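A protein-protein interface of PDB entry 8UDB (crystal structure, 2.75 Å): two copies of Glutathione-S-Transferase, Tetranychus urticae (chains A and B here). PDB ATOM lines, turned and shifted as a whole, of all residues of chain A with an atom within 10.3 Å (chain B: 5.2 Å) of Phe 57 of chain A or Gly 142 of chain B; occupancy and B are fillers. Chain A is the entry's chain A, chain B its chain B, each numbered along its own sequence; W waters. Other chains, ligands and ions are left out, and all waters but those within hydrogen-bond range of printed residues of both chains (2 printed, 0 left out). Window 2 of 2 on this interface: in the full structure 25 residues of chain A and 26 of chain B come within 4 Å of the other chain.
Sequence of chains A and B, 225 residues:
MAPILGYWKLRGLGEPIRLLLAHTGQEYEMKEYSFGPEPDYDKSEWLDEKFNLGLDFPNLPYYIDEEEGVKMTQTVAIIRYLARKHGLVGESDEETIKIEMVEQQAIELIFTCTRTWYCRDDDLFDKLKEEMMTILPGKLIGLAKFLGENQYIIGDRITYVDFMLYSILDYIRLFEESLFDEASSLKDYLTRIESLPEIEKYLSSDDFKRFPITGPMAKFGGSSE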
ATOM      1  N   TRP A  46     -13.273  18.783 -23.520  1.00  0.00           N
ATOM      2  CA  TRP A  46     -12.705  18.478 -22.217  1.00  0.00           C
ATOM      3  C   TRP A  46     -11.222  18.846 -22.143  1.00  0.00           C
ATOM      4  O   TRP A  46     -10.812  19.487 -21.175  1.00  0.00           O
ATOM      5  CB  TRP A  46     -12.941  16.999 -21.882  1.00  0.00           C
ATOM      6  CG  TRP A  46     -12.174  16.477 -20.703  1.00  0.00           C
ATOM      7  CD1 TRP A  46     -11.290  15.431 -20.688  1.00  0.00           C
ATOM      8  CD2 TRP A  46     -12.194  17.005 -19.365  1.00  0.00           C
ATOM      9  NE1 TRP A  46     -10.753  15.283 -19.439  1.00  0.00           N
ATOM     10  CE2 TRP A  46     -11.299  16.221 -18.603  1.00  0.00           C
ATOM     11  CE3 TRP A  46     -12.858  18.068 -18.742  1.00  0.00           C
ATOM     12  CZ2 TRP A  46     -11.080  16.449 -17.245  1.00  0.00           C
ATOM     13  CZ3 TRP A  46     -12.646  18.285 -17.398  1.00  0.00           C
ATOM     14  CH2 TRP A  46     -11.774  17.483 -16.663  1.00  0.00           C
ATOM     15  N   GLU A  49      -9.829  22.170 -21.276  1.00  0.00           N
ATOM     16  CA  GLU A  49     -10.096  22.689 -19.906  1.00  0.00           C
ATOM     17  C   GLU A  49      -9.557  21.716 -18.853  1.00  0.00           C
ATOM     18  O   GLU A  49      -9.421  22.133 -17.691  1.00  0.00           O
ATOM     19  CB  GLU A  49     -11.604  22.872 -19.742  1.00  0.00           C
ATOM     20  CG  GLU A  49     -12.000  23.651 -18.503  1.00  0.00           C
ATOM     21  CD  GLU A  49     -13.494  23.883 -18.365  1.00  0.00           C
ATOM     22  OE1 GLU A  49     -14.245  23.429 -19.248  1.00  0.00           O
ATOM     23  OE2 GLU A  49     -13.901  24.521 -17.376  1.00  0.00           O
ATOM     24  N   LYS A  50      -9.243  20.483 -19.252  1.00  0.00           N
ATOM     25  CA  LYS A  50      -8.781  19.424 -18.313  1.00  0.00           C
ATOM     26  C   LYS A  50      -7.814  19.937 -17.242  1.00  0.00           C
ATOM     27  O   LYS A  50      -7.940  19.483 -16.093  1.00  0.00           O
ATOM     28  CB  LYS A  50      -8.095  18.321 -19.123  1.00  0.00           C
ATOM     29  CG  LYS A  50      -7.564  17.140 -18.323  1.00  0.00           C
ATOM     30  CD  LYS A  50      -7.056  16.022 -19.201  1.00  0.00           C
ATOM     31  CE  LYS A  50      -6.522  14.849 -18.409  1.00  0.00           C
ATOM     32  NZ  LYS A  50      -6.123  13.731 -19.297  1.00  0.00           N
ATOM     33  N   PHE A  51      -6.904  20.853 -17.574  1.00  0.00           N
ATOM     34  CA  PHE A  51      -5.873  21.229 -16.614  1.00  0.00           C
ATOM     35  C   PHE A  51      -6.139  22.605 -15.995  1.00  0.00           C
ATOM     36  O   PHE A  51      -5.314  23.090 -15.232  1.00  0.00           O
ATOM     37  CB  PHE A  51      -4.490  21.165 -17.280  1.00  0.00           C
ATOM     38  CG  PHE A  51      -4.126  19.797 -17.817  1.00  0.00           C
ATOM     39  CD1 PHE A  51      -3.806  18.747 -16.955  1.00  0.00           C
ATOM     40  CD2 PHE A  51      -4.148  19.538 -19.182  1.00  0.00           C
ATOM     41  CE1 PHE A  51      -3.502  17.483 -17.444  1.00  0.00           C
ATOM     42  CE2 PHE A  51      -3.862  18.267 -19.669  1.00  0.00           C
ATOM     43  CZ  PHE A  51      -3.531  17.244 -18.801  1.00  0.00           C
ATOM     44  N   ASN A  52      -7.311  23.203 -16.239  1.00  0.00           N
ATOM     45  CA  ASN A  52      -7.547  24.574 -15.819  1.00  0.00           C
ATOM     46  C   ASN A  52      -8.529  24.661 -14.653  1.00  0.00           C
ATOM     47  O   ASN A  52      -8.917  25.774 -14.296  1.00  0.00           O
ATOM     48  CB  ASN A  52      -8.094  25.441 -16.957  1.00  0.00           C
ATOM     49  CG  ASN A  52      -7.227  25.457 -18.198  1.00  0.00           C
ATOM     50  OD1 ASN A  52      -6.075  25.019 -18.189  1.00  0.00           O
ATOM     51  ND2 ASN A  52      -7.787  25.974 -19.276  1.00  0.00           N
ATOM     52  N   LEU A  53      -8.895  23.518 -14.046  1.00  0.00           N
ATOM     53  CA  LEU A  53      -9.925  23.483 -13.019  1.00  0.00           C
ATOM     54  C   LEU A  53      -9.342  23.254 -11.622  1.00  0.00           C
ATOM     55  O   LEU A  53     -10.100  23.187 -10.647  1.00  0.00           O
ATOM     56  CB  LEU A  53     -10.898  22.365 -13.394  1.00  0.00           C
ATOM     57  CG  LEU A  53     -11.944  22.730 -14.442  1.00  0.00           C
ATOM     58  CD1 LEU A  53     -12.637  21.484 -14.962  1.00  0.00           C
ATOM     59  CD2 LEU A  53     -12.968  23.701 -13.861  1.00  0.00           C
ATOM     60  N   GLY A  54      -8.012  23.096 -11.542  1.00  0.00           N
ATOM     61  CA  GLY A  54      -7.323  22.927 -10.273  1.00  0.00           C
ATOM     62  C   GLY A  54      -7.423  21.515  -9.681  1.00  0.00           C
ATOM     63  O   GLY A  54      -7.026  21.303  -8.539  1.00  0.00           O
ATOM     64  N   LEU A  55      -7.912  20.544 -10.468  1.00  0.00           N
ATOM     65  CA  LEU A  55      -8.061  19.155 -10.046  1.00  0.00           C
ATOM     66  C   LEU A  55      -6.700  18.475  -9.940  1.00  0.00           C
ATOM     67  O   LEU A  55      -5.856  18.656 -10.798  1.00  0.00           O
ATOM     68  CB  LEU A  55      -8.908  18.422 -11.087  1.00  0.00           C
ATOM     69  CG  LEU A  55     -10.291  19.013 -11.328  1.00  0.00           C
ATOM     70  CD1 LEU A  55     -10.899  18.434 -12.599  1.00  0.00           C
ATOM     71  CD2 LEU A  55     -11.188  18.780 -10.116  1.00  0.00           C
ATOM     72  N   ASP A  56      -6.514  17.645  -8.913  1.00  0.00           N
ATOM     73  CA  ASP A  56      -5.266  16.921  -8.735  1.00  0.00           C
ATOM     74  C   ASP A  56      -5.128  15.835  -9.797  1.00  0.00           C
ATOM     75  O   ASP A  56      -4.055  15.709 -10.384  1.00  0.00           O
ATOM     76  CB  ASP A  56      -5.179  16.232  -7.379  1.00  0.00           C
ATOM     77  CG  ASP A  56      -5.357  17.151  -6.195  1.00  0.00           C
ATOM     78  OD1 ASP A  56      -4.491  18.054  -6.044  1.00  0.00           O
ATOM     79  OD2 ASP A  56      -6.364  16.943  -5.443  1.00  0.00           O
ATOM     80  N   PHE A  57      -6.198  15.033  -9.990  1.00  0.00           N
ATOM     81  CA  PHE A  57      -6.193  13.927 -10.943  1.00  0.00           C
ATOM     82  C   PHE A  57      -7.257  14.195 -11.995  1.00  0.00           C
ATOM     83  O   PHE A  57      -8.310  13.567 -11.971  1.00  0.00           O
ATOM     84  CB  PHE A  57      -6.416  12.580 -10.246  1.00  0.00           C
ATOM     85  CG  PHE A  57      -5.403  12.315  -9.163  1.00  0.00           C
ATOM     86  CD1 PHE A  57      -4.050  12.216  -9.468  1.00  0.00           C
ATOM     87  CD2 PHE A  57      -5.789  12.242  -7.831  1.00  0.00           C
ATOM     88  CE1 PHE A  57      -3.107  12.004  -8.471  1.00  0.00           C
ATOM     89  CE2 PHE A  57      -4.845  12.033  -6.834  1.00  0.00           C
ATOM     90  CZ  PHE A  57      -3.506  11.915  -7.155  1.00  0.00           C
ATOM     91  N   PRO A  58      -6.994  15.148 -12.924  1.00  0.00           N
ATOM     92  CA  PRO A  58      -8.015  15.663 -13.839  1.00  0.00           C
ATOM     93  C   PRO A  58      -8.688  14.549 -14.632  1.00  0.00           C
ATOM     94  O   PRO A  58      -8.031  13.737 -15.284  1.00  0.00           O
ATOM     95  CB  PRO A  58      -7.266  16.672 -14.732  1.00  0.00           C
ATOM     96  CG  PRO A  58      -5.789  16.409 -14.504  1.00  0.00           C
ATOM     97  CD  PRO A  58      -5.691  15.823 -13.115  1.00  0.00           C
ATOM     98  N   ASN A  59     -10.018  14.496 -14.513  1.00  0.00           N
ATOM     99  CA  ASN A  59     -10.807  13.386 -15.018  1.00  0.00           C
ATOM    100  C   ASN A  59     -12.278  13.793 -15.022  1.00  0.00           C
ATOM    101  O   ASN A  59     -12.665  14.790 -14.410  1.00  0.00           O
ATOM    102  CB  ASN A  59     -10.580  12.100 -14.216  1.00  0.00           C
ATOM    103  CG  ASN A  59     -10.463  10.879 -15.108  1.00  0.00           C
ATOM    104  OD1 ASN A  59     -11.069  10.827 -16.176  1.00  0.00           O
ATOM    105  ND2 ASN A  59      -9.633   9.916 -14.725  1.00  0.00           N
ATOM    106  N   LEU A  60     -13.073  13.035 -15.784  1.00  0.00           N
ATOM    107  CA  LEU A  60     -14.521  13.163 -15.782  1.00  0.00           C
ATOM    108  C   LEU A  60     -15.084  11.837 -15.292  1.00  0.00           C
ATOM    109  O   LEU A  60     -14.733  10.799 -15.850  1.00  0.00           O
ATOM    110  CB  LEU A  60     -15.056  13.477 -17.185  1.00  0.00           C
ATOM    111  CG  LEU A  60     -14.788  14.877 -17.737  1.00  0.00           C
ATOM    112  CD1 LEU A  60     -15.455  15.046 -19.094  1.00  0.00           C
ATOM    113  CD2 LEU A  60     -15.295  15.953 -16.807  1.00  0.00           C
ATOM    114  N   PRO A  61     -15.989  11.834 -14.283  1.00  0.00           N
ATOM    115  CA  PRO A  61     -16.543  13.058 -13.710  1.00  0.00           C
ATOM    116  C   PRO A  61     -15.677  13.718 -12.639  1.00  0.00           C
ATOM    117  O   PRO A  61     -14.727  13.101 -12.126  1.00  0.00           O
ATOM    118  CB  PRO A  61     -17.846  12.546 -13.073  1.00  0.00           C
ATOM    119  CG  PRO A  61     -17.463  11.190 -12.557  1.00  0.00           C
ATOM    120  CD  PRO A  61     -16.575  10.637 -13.660  1.00  0.00           C
ATOM    121  N   TYR A  62     -16.039  14.973 -12.326  1.00  0.00           N
ATOM    122  CA  TYR A  62     -15.445  15.712 -11.224  1.00  0.00           C
ATOM    123  C   TYR A  62     -16.546  16.402 -10.420  1.00  0.00           C
ATOM    124  O   TYR A  62     -17.642  16.639 -10.914  1.00  0.00           O
ATOM    125  CB  TYR A  62     -14.398  16.716 -11.726  1.00  0.00           C
ATOM    126  CG  TYR A  62     -14.922  17.861 -12.556  1.00  0.00           C
ATOM    127  CD1 TYR A  62     -15.727  18.852 -12.011  1.00  0.00           C
ATOM    128  CD2 TYR A  62     -14.606  17.966 -13.903  1.00  0.00           C
ATOM    129  CE1 TYR A  62     -16.205  19.909 -12.777  1.00  0.00           C
ATOM    130  CE2 TYR A  62     -15.086  19.005 -14.691  1.00  0.00           C
ATOM    131  CZ  TYR A  62     -15.884  19.985 -14.126  1.00  0.00           C
ATOM    132  OH  TYR A  62     -16.334  20.998 -14.937  1.00  0.00           O
ATOM    133  N   TYR A  63     -16.228  16.730  -9.174  1.00  0.00           N
ATOM    134  CA  TYR A  63     -17.174  17.374  -8.284  1.00  0.00           C
ATOM    135  C   TYR A  63     -16.448  18.500  -7.554  1.00  0.00           C
ATOM    136  O   TYR A  63     -15.390  18.296  -6.937  1.00  0.00           O
ATOM    137  CB  TYR A  63     -17.798  16.361  -7.319  1.00  0.00           C
ATOM    138  CG  TYR A  63     -18.797  16.949  -6.357  1.00  0.00           C
ATOM    139  CD1 TYR A  63     -20.142  17.061  -6.688  1.00  0.00           C
ATOM    140  CD2 TYR A  63     -18.397  17.404  -5.114  1.00  0.00           C
ATOM    141  CE1 TYR A  63     -21.062  17.618  -5.814  1.00  0.00           C
ATOM    142  CE2 TYR A  63     -19.304  17.958  -4.229  1.00  0.00           C
ATOM    143  CZ  TYR A  63     -20.640  18.058  -4.573  1.00  0.00           C
ATOM    144  OH  TYR A  63     -21.526  18.623  -3.687  1.00  0.00           O
ATOM    145  N   LYS A  71     -12.742  19.691  -4.135  1.00  0.00           N
ATOM    146  CA  LYS A  71     -12.392  19.638  -5.555  1.00  0.00           C
ATOM    147  C   LYS A  71     -11.884  18.244  -5.914  1.00  0.00           C
ATOM    148  O   LYS A  71     -10.707  17.963  -5.707  1.00  0.00           O
ATOM    149  CB  LYS A  71     -11.267  20.621  -5.895  1.00  0.00           C
ATOM    150  CG  LYS A  71     -11.719  21.914  -6.541  1.00  0.00           C
ATOM    151  CD  LYS A  71     -10.568  22.845  -6.816  1.00  0.00           C
ATOM    152  CE  LYS A  71     -11.000  24.291  -6.746  1.00  0.00           C
ATOM    153  NZ  LYS A  71      -9.863  25.194  -7.031  1.00  0.00           N
ATOM    154  N   MET A  72     -12.783  17.333  -6.309  1.00  0.00           N
ATOM    155  CA  MET A  72     -12.391  15.905  -6.485  1.00  0.00           C
ATOM    156  C   MET A  72     -12.665  15.394  -7.901  1.00  0.00           C
ATOM    157  O   MET A  72     -13.382  16.079  -8.641  1.00  0.00           O
ATOM    158  CB  MET A  72     -13.222  15.034  -5.542  1.00  0.00           C
ATOM    159  CG  MET A  72     -13.260  15.500  -4.110  1.00  0.00           C
ATOM    160  SD  MET A  72     -14.503  14.560  -3.192  1.00  0.00           S
ATOM    161  CE  MET A  72     -15.829  14.532  -4.394  1.00  0.00           C
ATOM    162  N   THR A  73     -12.144  14.198  -8.229  1.00  0.00           N
ATOM    163  CA  THR A  73     -12.330  13.677  -9.608  1.00  0.00           C
ATOM    164  C   THR A  73     -12.519  12.162  -9.718  1.00  0.00           C
ATOM    165  O   THR A  73     -12.408  11.680 -10.851  1.00  0.00           O
ATOM    166  CB  THR A  73     -11.104  13.944 -10.488  1.00  0.00           C
ATOM    167  OG1 THR A  73      -9.939  13.641  -9.723  1.00  0.00           O
ATOM    168  CG2 THR A  73     -11.041  15.363 -11.000  1.00  0.00           C
ATOM    169  N   GLN A  74     -12.794  11.419  -8.647  1.00  0.00           N
ATOM    170  CA  GLN A  74     -12.975   9.955  -8.881  1.00  0.00           C
ATOM    171  C   GLN A  74     -14.413   9.535  -8.559  1.00  0.00           C
ATOM    172  O   GLN A  74     -14.836   9.758  -7.422  1.00  0.00           O
ATOM    173  CB  GLN A  74     -11.927   9.146  -8.114  1.00  0.00           C
ATOM    174  CG  GLN A  74     -10.493   9.393  -8.561  1.00  0.00           C
ATOM    175  CD  GLN A  74     -10.235   8.949  -9.980  1.00  0.00           C
ATOM    176  OE1 GLN A  74     -10.443   7.792 -10.338  1.00  0.00           O
ATOM    177  NE2 GLN A  74      -9.773   9.874 -10.804  1.00  0.00           N
ATOM    178  N   THR A  75     -15.112   8.901  -9.502  1.00  0.00           N
ATOM    179  CA  THR A  75     -16.545   8.533  -9.321  1.00  0.00           C
ATOM    180  C   THR A  75     -16.821   7.942  -7.936  1.00  0.00           C
ATOM    181  O   THR A  75     -17.695   8.483  -7.243  1.00  0.00           O
ATOM    182  CB  THR A  75     -16.995   7.544 -10.403  1.00  0.00           C
ATOM    183  OG1 THR A  75     -16.624   8.064 -11.678  1.00  0.00           O
ATOM    184  CG2 THR A  75     -18.483   7.273 -10.373  1.00  0.00           C
ATOM    185  N   ALA A  77     -14.974   7.903  -5.231  1.00  0.00           N
ATOM    186  CA  ALA A  77     -14.592   8.866  -4.181  1.00  0.00           C
ATOM    187  C   ALA A  77     -15.659   9.954  -4.092  1.00  0.00           C
ATOM    188  O   ALA A  77     -15.923  10.434  -2.982  1.00  0.00           O
ATOM    189  CB  ALA A  77     -13.242   9.439  -4.506  1.00  0.00           C
ATOM    190  N   ILE A  78     -16.257  10.310  -5.226  1.00  0.00           N
ATOM    191  CA  ILE A  78     -17.245  11.375  -5.243  1.00  0.00           C
ATOM    192  C   ILE A  78     -18.508  10.882  -4.546  1.00  0.00           C
ATOM    193  O   ILE A  78     -19.063  11.560  -3.668  1.00  0.00           O
ATOM    194  CB  ILE A  78     -17.517  11.859  -6.681  1.00  0.00           C
ATOM    195  CG1 ILE A  78     -16.261  12.444  -7.335  1.00  0.00           C
ATOM    196  CG2 ILE A  78     -18.658  12.856  -6.703  1.00  0.00           C
ATOM    197  CD1 ILE A  78     -16.454  12.867  -8.770  1.00  0.00           C
ATOM    198  N   MET B 101      -9.270   9.176  -3.567  1.00  0.00           N
ATOM    199  CA  MET B 101      -8.945   9.604  -4.917  1.00  0.00           C
ATOM    200  C   MET B 101      -7.758   8.786  -5.424  1.00  0.00           C
ATOM    201  O   MET B 101      -7.768   8.258  -6.538  1.00  0.00           O
ATOM    202  CB  MET B 101      -8.637  11.105  -4.936  1.00  0.00           C
ATOM    203  CG  MET B 101      -9.905  11.942  -5.036  1.00  0.00           C
ATOM    204  SD  MET B 101      -9.689  13.649  -5.640  1.00  0.00           S
ATOM    205  CE  MET B 101      -8.711  14.394  -4.330  1.00  0.00           C
ATOM    206  N   VAL B 102      -6.751   8.658  -4.555  1.00  0.00           N
ATOM    207  CA  VAL B 102      -5.521   7.962  -4.888  1.00  0.00           C
ATOM    208  C   VAL B 102      -5.813   6.472  -5.086  1.00  0.00           C
ATOM    209  O   VAL B 102      -5.326   5.854  -6.028  1.00  0.00           O
ATOM    210  CB  VAL B 102      -4.483   8.198  -3.781  1.00  0.00           C
ATOM    211  CG1 VAL B 102      -3.313   7.245  -3.904  1.00  0.00           C
ATOM    212  CG2 VAL B 102      -3.998   9.634  -3.730  1.00  0.00           C
ATOM    213  N   GLN B 105      -7.442   6.252  -8.386  1.00  0.00           N
ATOM    214  CA  GLN B 105      -6.451   6.511  -9.413  1.00  0.00           C
ATOM    215  C   GLN B 105      -5.561   5.278  -9.574  1.00  0.00           C
ATOM    216  O   GLN B 105      -5.157   4.960 -10.685  1.00  0.00           O
ATOM    217  CB  GLN B 105      -5.666   7.783  -9.084  1.00  0.00           C
ATOM    218  CG  GLN B 105      -4.576   8.115 -10.102  1.00  0.00           C
ATOM    219  CD  GLN B 105      -5.079   8.467 -11.484  1.00  0.00           C
ATOM    220  OE1 GLN B 105      -5.808   9.443 -11.658  1.00  0.00           O
ATOM    221  NE2 GLN B 105      -4.698   7.656 -12.466  1.00  0.00           N
ATOM    222  N   PRO B 137       2.455   8.660 -18.997  1.00  0.00           N
ATOM    223  CA  PRO B 137       3.340   9.706 -18.494  1.00  0.00           C
ATOM    224  C   PRO B 137       2.581  10.795 -17.751  1.00  0.00           C
ATOM    225  O   PRO B 137       3.037  11.232 -16.698  1.00  0.00           O
ATOM    226  CB  PRO B 137       4.015  10.242 -19.766  1.00  0.00           C
ATOM    227  CG  PRO B 137       4.069   9.045 -20.667  1.00  0.00           C
ATOM    228  CD  PRO B 137       2.751   8.344 -20.407  1.00  0.00           C
ATOM    229  N   GLY B 138       1.427  11.205 -18.309  1.00  0.00           N
ATOM    230  CA  GLY B 138       0.571  12.230 -17.723  1.00  0.00           C
ATOM    231  C   GLY B 138       0.012  11.843 -16.350  1.00  0.00           C
ATOM    232  O   GLY B 138      -0.152  12.701 -15.478  1.00  0.00           O
ATOM    233  N   LYS B 139      -0.282  10.549 -16.163  1.00  0.00           N
ATOM    234  CA  LYS B 139      -0.859  10.083 -14.912  1.00  0.00           C
ATOM    235  C   LYS B 139       0.201  10.061 -13.820  1.00  0.00           C
ATOM    236  O   LYS B 139      -0.099  10.360 -12.663  1.00  0.00           O
ATOM    237  CB  LYS B 139      -1.417   8.664 -15.050  1.00  0.00           C
ATOM    238  CG  LYS B 139      -2.468   8.485 -16.131  1.00  0.00           C
ATOM    239  CD  LYS B 139      -3.748   9.182 -15.782  1.00  0.00           C
ATOM    240  CE  LYS B 139      -4.735   9.139 -16.926  1.00  0.00           C
ATOM    241  NZ  LYS B 139      -6.106   9.409 -16.452  1.00  0.00           N
ATOM    242  N   LEU B 140       1.413   9.639 -14.214  1.00  0.00           N
ATOM    243  CA  LEU B 140       2.541   9.508 -13.301  1.00  0.00           C
ATOM    244  C   LEU B 140       2.994  10.892 -12.860  1.00  0.00           C
ATOM    245  O   LEU B 140       3.347  11.081 -11.700  1.00  0.00           O
ATOM    246  CB  LEU B 140       3.671   8.738 -13.995  1.00  0.00           C
ATOM    247  CG  LEU B 140       3.360   7.278 -14.318  1.00  0.00           C
ATOM    248  CD1 LEU B 140       4.470   6.631 -15.114  1.00  0.00           C
ATOM    249  CD2 LEU B 140       3.101   6.472 -13.049  1.00  0.00           C
ATOM    250  N   ILE B 141       2.960  11.841 -13.800  1.00  0.00           N
ATOM    251  CA  ILE B 141       3.282  13.214 -13.480  1.00  0.00           C
ATOM    252  C   ILE B 141       2.233  13.753 -12.501  1.00  0.00           C
ATOM    253  O   ILE B 141       2.587  14.457 -11.567  1.00  0.00           O
ATOM    254  CB  ILE B 141       3.443  14.059 -14.766  1.00  0.00           C
ATOM    255  CG1 ILE B 141       4.659  13.589 -15.572  1.00  0.00           C
ATOM    256  CG2 ILE B 141       3.528  15.546 -14.432  1.00  0.00           C
ATOM    257  CD1 ILE B 141       4.684  14.015 -17.036  1.00  0.00           C
ATOM    258  N   GLY B 142       0.950  13.414 -12.685  1.00  0.00           N
ATOM    259  CA  GLY B 142      -0.089  13.858 -11.766  1.00  0.00           C
ATOM    260  C   GLY B 142       0.165  13.362 -10.343  1.00  0.00           C
ATOM    261  O   GLY B 142      -0.046  14.077  -9.360  1.00  0.00           O
ATOM    262  N   LEU B 143       0.647  12.120 -10.264  1.00  0.00           N
ATOM    263  CA  LEU B 143       0.915  11.457  -9.005  1.00  0.00           C
ATOM    264  C   LEU B 143       2.135  12.075  -8.332  1.00  0.00           C
ATOM    265  O   LEU B 143       2.113  12.308  -7.121  1.00  0.00           O
ATOM    266  CB  LEU B 143       1.123   9.969  -9.295  1.00  0.00           C
ATOM    267  CG  LEU B 143      -0.176   9.195  -9.500  1.00  0.00           C
ATOM    268  CD1 LEU B 143       0.050   7.851 -10.159  1.00  0.00           C
ATOM    269  CD2 LEU B 143      -0.850   8.994  -8.160  1.00  0.00           C
ATOM    270  N   ALA B 144       3.190  12.313  -9.123  1.00  0.00           N
ATOM    271  CA  ALA B 144       4.410  12.931  -8.632  1.00  0.00           C
ATOM    272  C   ALA B 144       4.103  14.314  -8.066  1.00  0.00           C
ATOM    273  O   ALA B 144       4.624  14.678  -7.011  1.00  0.00           O
ATOM    274  CB  ALA B 144       5.428  13.008  -9.740  1.00  0.00           C
ATOM    275  N   LYS B 145       3.269  15.066  -8.784  1.00  0.00           N
ATOM    276  CA  LYS B 145       2.884  16.424  -8.327  1.00  0.00           C
ATOM    277  C   LYS B 145       2.106  16.291  -7.022  1.00  0.00           C
ATOM    278  O   LYS B 145       2.479  16.957  -6.044  1.00  0.00           O
ATOM    279  CB  LYS B 145       2.023  17.113  -9.387  1.00  0.00           C
ATOM    280  CG  LYS B 145       1.581  18.528  -9.047  1.00  0.00           C
ATOM    281  CD  LYS B 145       0.461  19.030  -9.929  1.00  0.00           C
ATOM    282  CE  LYS B 145      -0.143  20.325  -9.430  1.00  0.00           C
ATOM    283  NZ  LYS B 145      -1.395  20.659 -10.148  1.00  0.00           N
ATOM    284  N   PHE B 146       1.066  15.459  -7.023  1.00  0.00           N
ATOM    285  CA  PHE B 146       0.261  15.272  -5.827  1.00  0.00           C
ATOM    286  C   PHE B 146       1.148  14.904  -4.635  1.00  0.00           C
ATOM    287  O   PHE B 146       0.938  15.381  -3.536  1.00  0.00           O
ATOM    288  CB  PHE B 146      -0.814  14.215  -6.084  1.00  0.00           C
ATOM    289  CG  PHE B 146      -1.799  14.044  -4.956  1.00  0.00           C
ATOM    290  CD1 PHE B 146      -2.833  14.946  -4.758  1.00  0.00           C
ATOM    291  CD2 PHE B 146      -1.673  12.984  -4.071  1.00  0.00           C
ATOM    292  CE1 PHE B 146      -3.725  14.779  -3.704  1.00  0.00           C
ATOM    293  CE2 PHE B 146      -2.566  12.819  -3.025  1.00  0.00           C
ATOM    294  CZ  PHE B 146      -3.594  13.713  -2.845  1.00  0.00           C
ATOM    295  N   LEU B 147       2.142  14.049  -4.855  1.00  0.00           N
ATOM    296  CA  LEU B 147       3.039  13.613  -3.799  1.00  0.00           C
ATOM    297  C   LEU B 147       3.937  14.764  -3.339  1.00  0.00           C
ATOM    298  O   LEU B 147       4.079  14.985  -2.141  1.00  0.00           O
ATOM    299  CB  LEU B 147       3.867  12.449  -4.348  1.00  0.00           C
ATOM    300  CG  LEU B 147       5.034  11.984  -3.485  1.00  0.00           C
ATOM    301  CD1 LEU B 147       4.524  11.276  -2.247  1.00  0.00           C
ATOM    302  CD2 LEU B 147       5.950  11.083  -4.298  1.00  0.00           C
HETATM  303  O   HOH W   1      -8.821  15.746  -8.684  1.00  0.00           O
HETATM  304  O   HOH W   2      -1.821  15.949  -9.013  1.00  0.00           O
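Water W1 lies within hydrogen-bond range of the side-chain hydroxyl (OG1) of Thr 73 of chain A, the backbone NH (N) of Asp 56 of chain A, the backbone NH (N) of Phe 57 of chain A and the side-chain sulfur (SD) of Met 101 of chain B.
Water W2 bridges the backbone carbonyl oxygen of Gly 142 of chain B (2.6 Å) and the backbone carbonyl oxygen of Asp 56 of chain A (2.6 Å).
Among the printed residues, merely in contact across the chains: Asp 56 of chain A with Met 101 of chain B, Asp 56 of chain A with Phe 146 of chain B, Phe 57 of chain A with Gln 105 of chain B, Phe 57 of chain A with Gly 142 of chain B, Phe 57 of chain A with Leu 143 of chain B, Phe 57 of chain A with Phe 146 of chain B, Asn 59 of chain A with Lys 139 of chain B, Met 72 of chain A with Met 101 of chain B, Gln 74 of chain A with Met 101 of chain B and Gln 74 of chain A with Gln 105 of chain B.
Hydrophobic or aromatic side chains of chain B within 4 Å of the printed part of chain A: Met 101, Leu 143 and Phe 146.
Printed residues of chain A that touch a printed residue of chain B: Asp 56, Phe 57, Asn 59, Met 72, Thr 73 and Gln 74.
Hydrophobic or aromatic side chains of chain A that line the printed part of chain B: Phe 57 and Met 72.
No position is printed for both chains.
The side-chain hydroxyl (OG1) of Thr 73 of chain A is in hydrogen-bond range of the backbone carbonyl oxygen (O) of Phe 57 of chain A, 2.8 Å away.
The backbone carbonyl oxygen (O) of Tyr 63 of chain A sits at hydrogen-bond distance from the backbone NH (N) of Met 72 of chain A (2.8 Å).
The backbone NH of Thr 73 of chain A lies within hydrogen-bond range of the side-chain sulfur of Met 101 of chain B, at 3.6 Å.
Of the printed residues of chain B, Phe 57 of chain A touches Gln 105, Gly 142, Leu 143 and Phe 146.
Printed residues of chain A within 4 Å of Gly 142 of chain B: Phe 57.
Met 101 of chain B touches just these residues of chain A: Asp 56, Met 72, Thr 73 and Gln 74.
No residue of chain A comes within 4 Å of Gly 138 of chain B.
Of the printed residues of chain A, Leu 143 of chain B touches Phe 57 (3.8 Å).
No residue of chain A comes within 4 Å of Ala 144 of chain B.
Of chain A, only Asp 56 (3.6 Å) and Phe 57 (3.5 Å) come within 4 Å of Phe 146 of chain B.
Of the printed residues of chain B, Asp 56 of chain A touches Met 101 and Phe 146.
Of the printed residues of chain B, Met 72 of chain A touches Met 101.
Printed residues of chain B within 4 Å of Thr 73 of chain A: Met 101.
Of the printed residues of chain A, Lys 139 of chain B touches Asn 59.
Phe 51 of chain A touches none of the printed residues of chain B.
Thr 75 of chain A touches none of the printed residues of chain B.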
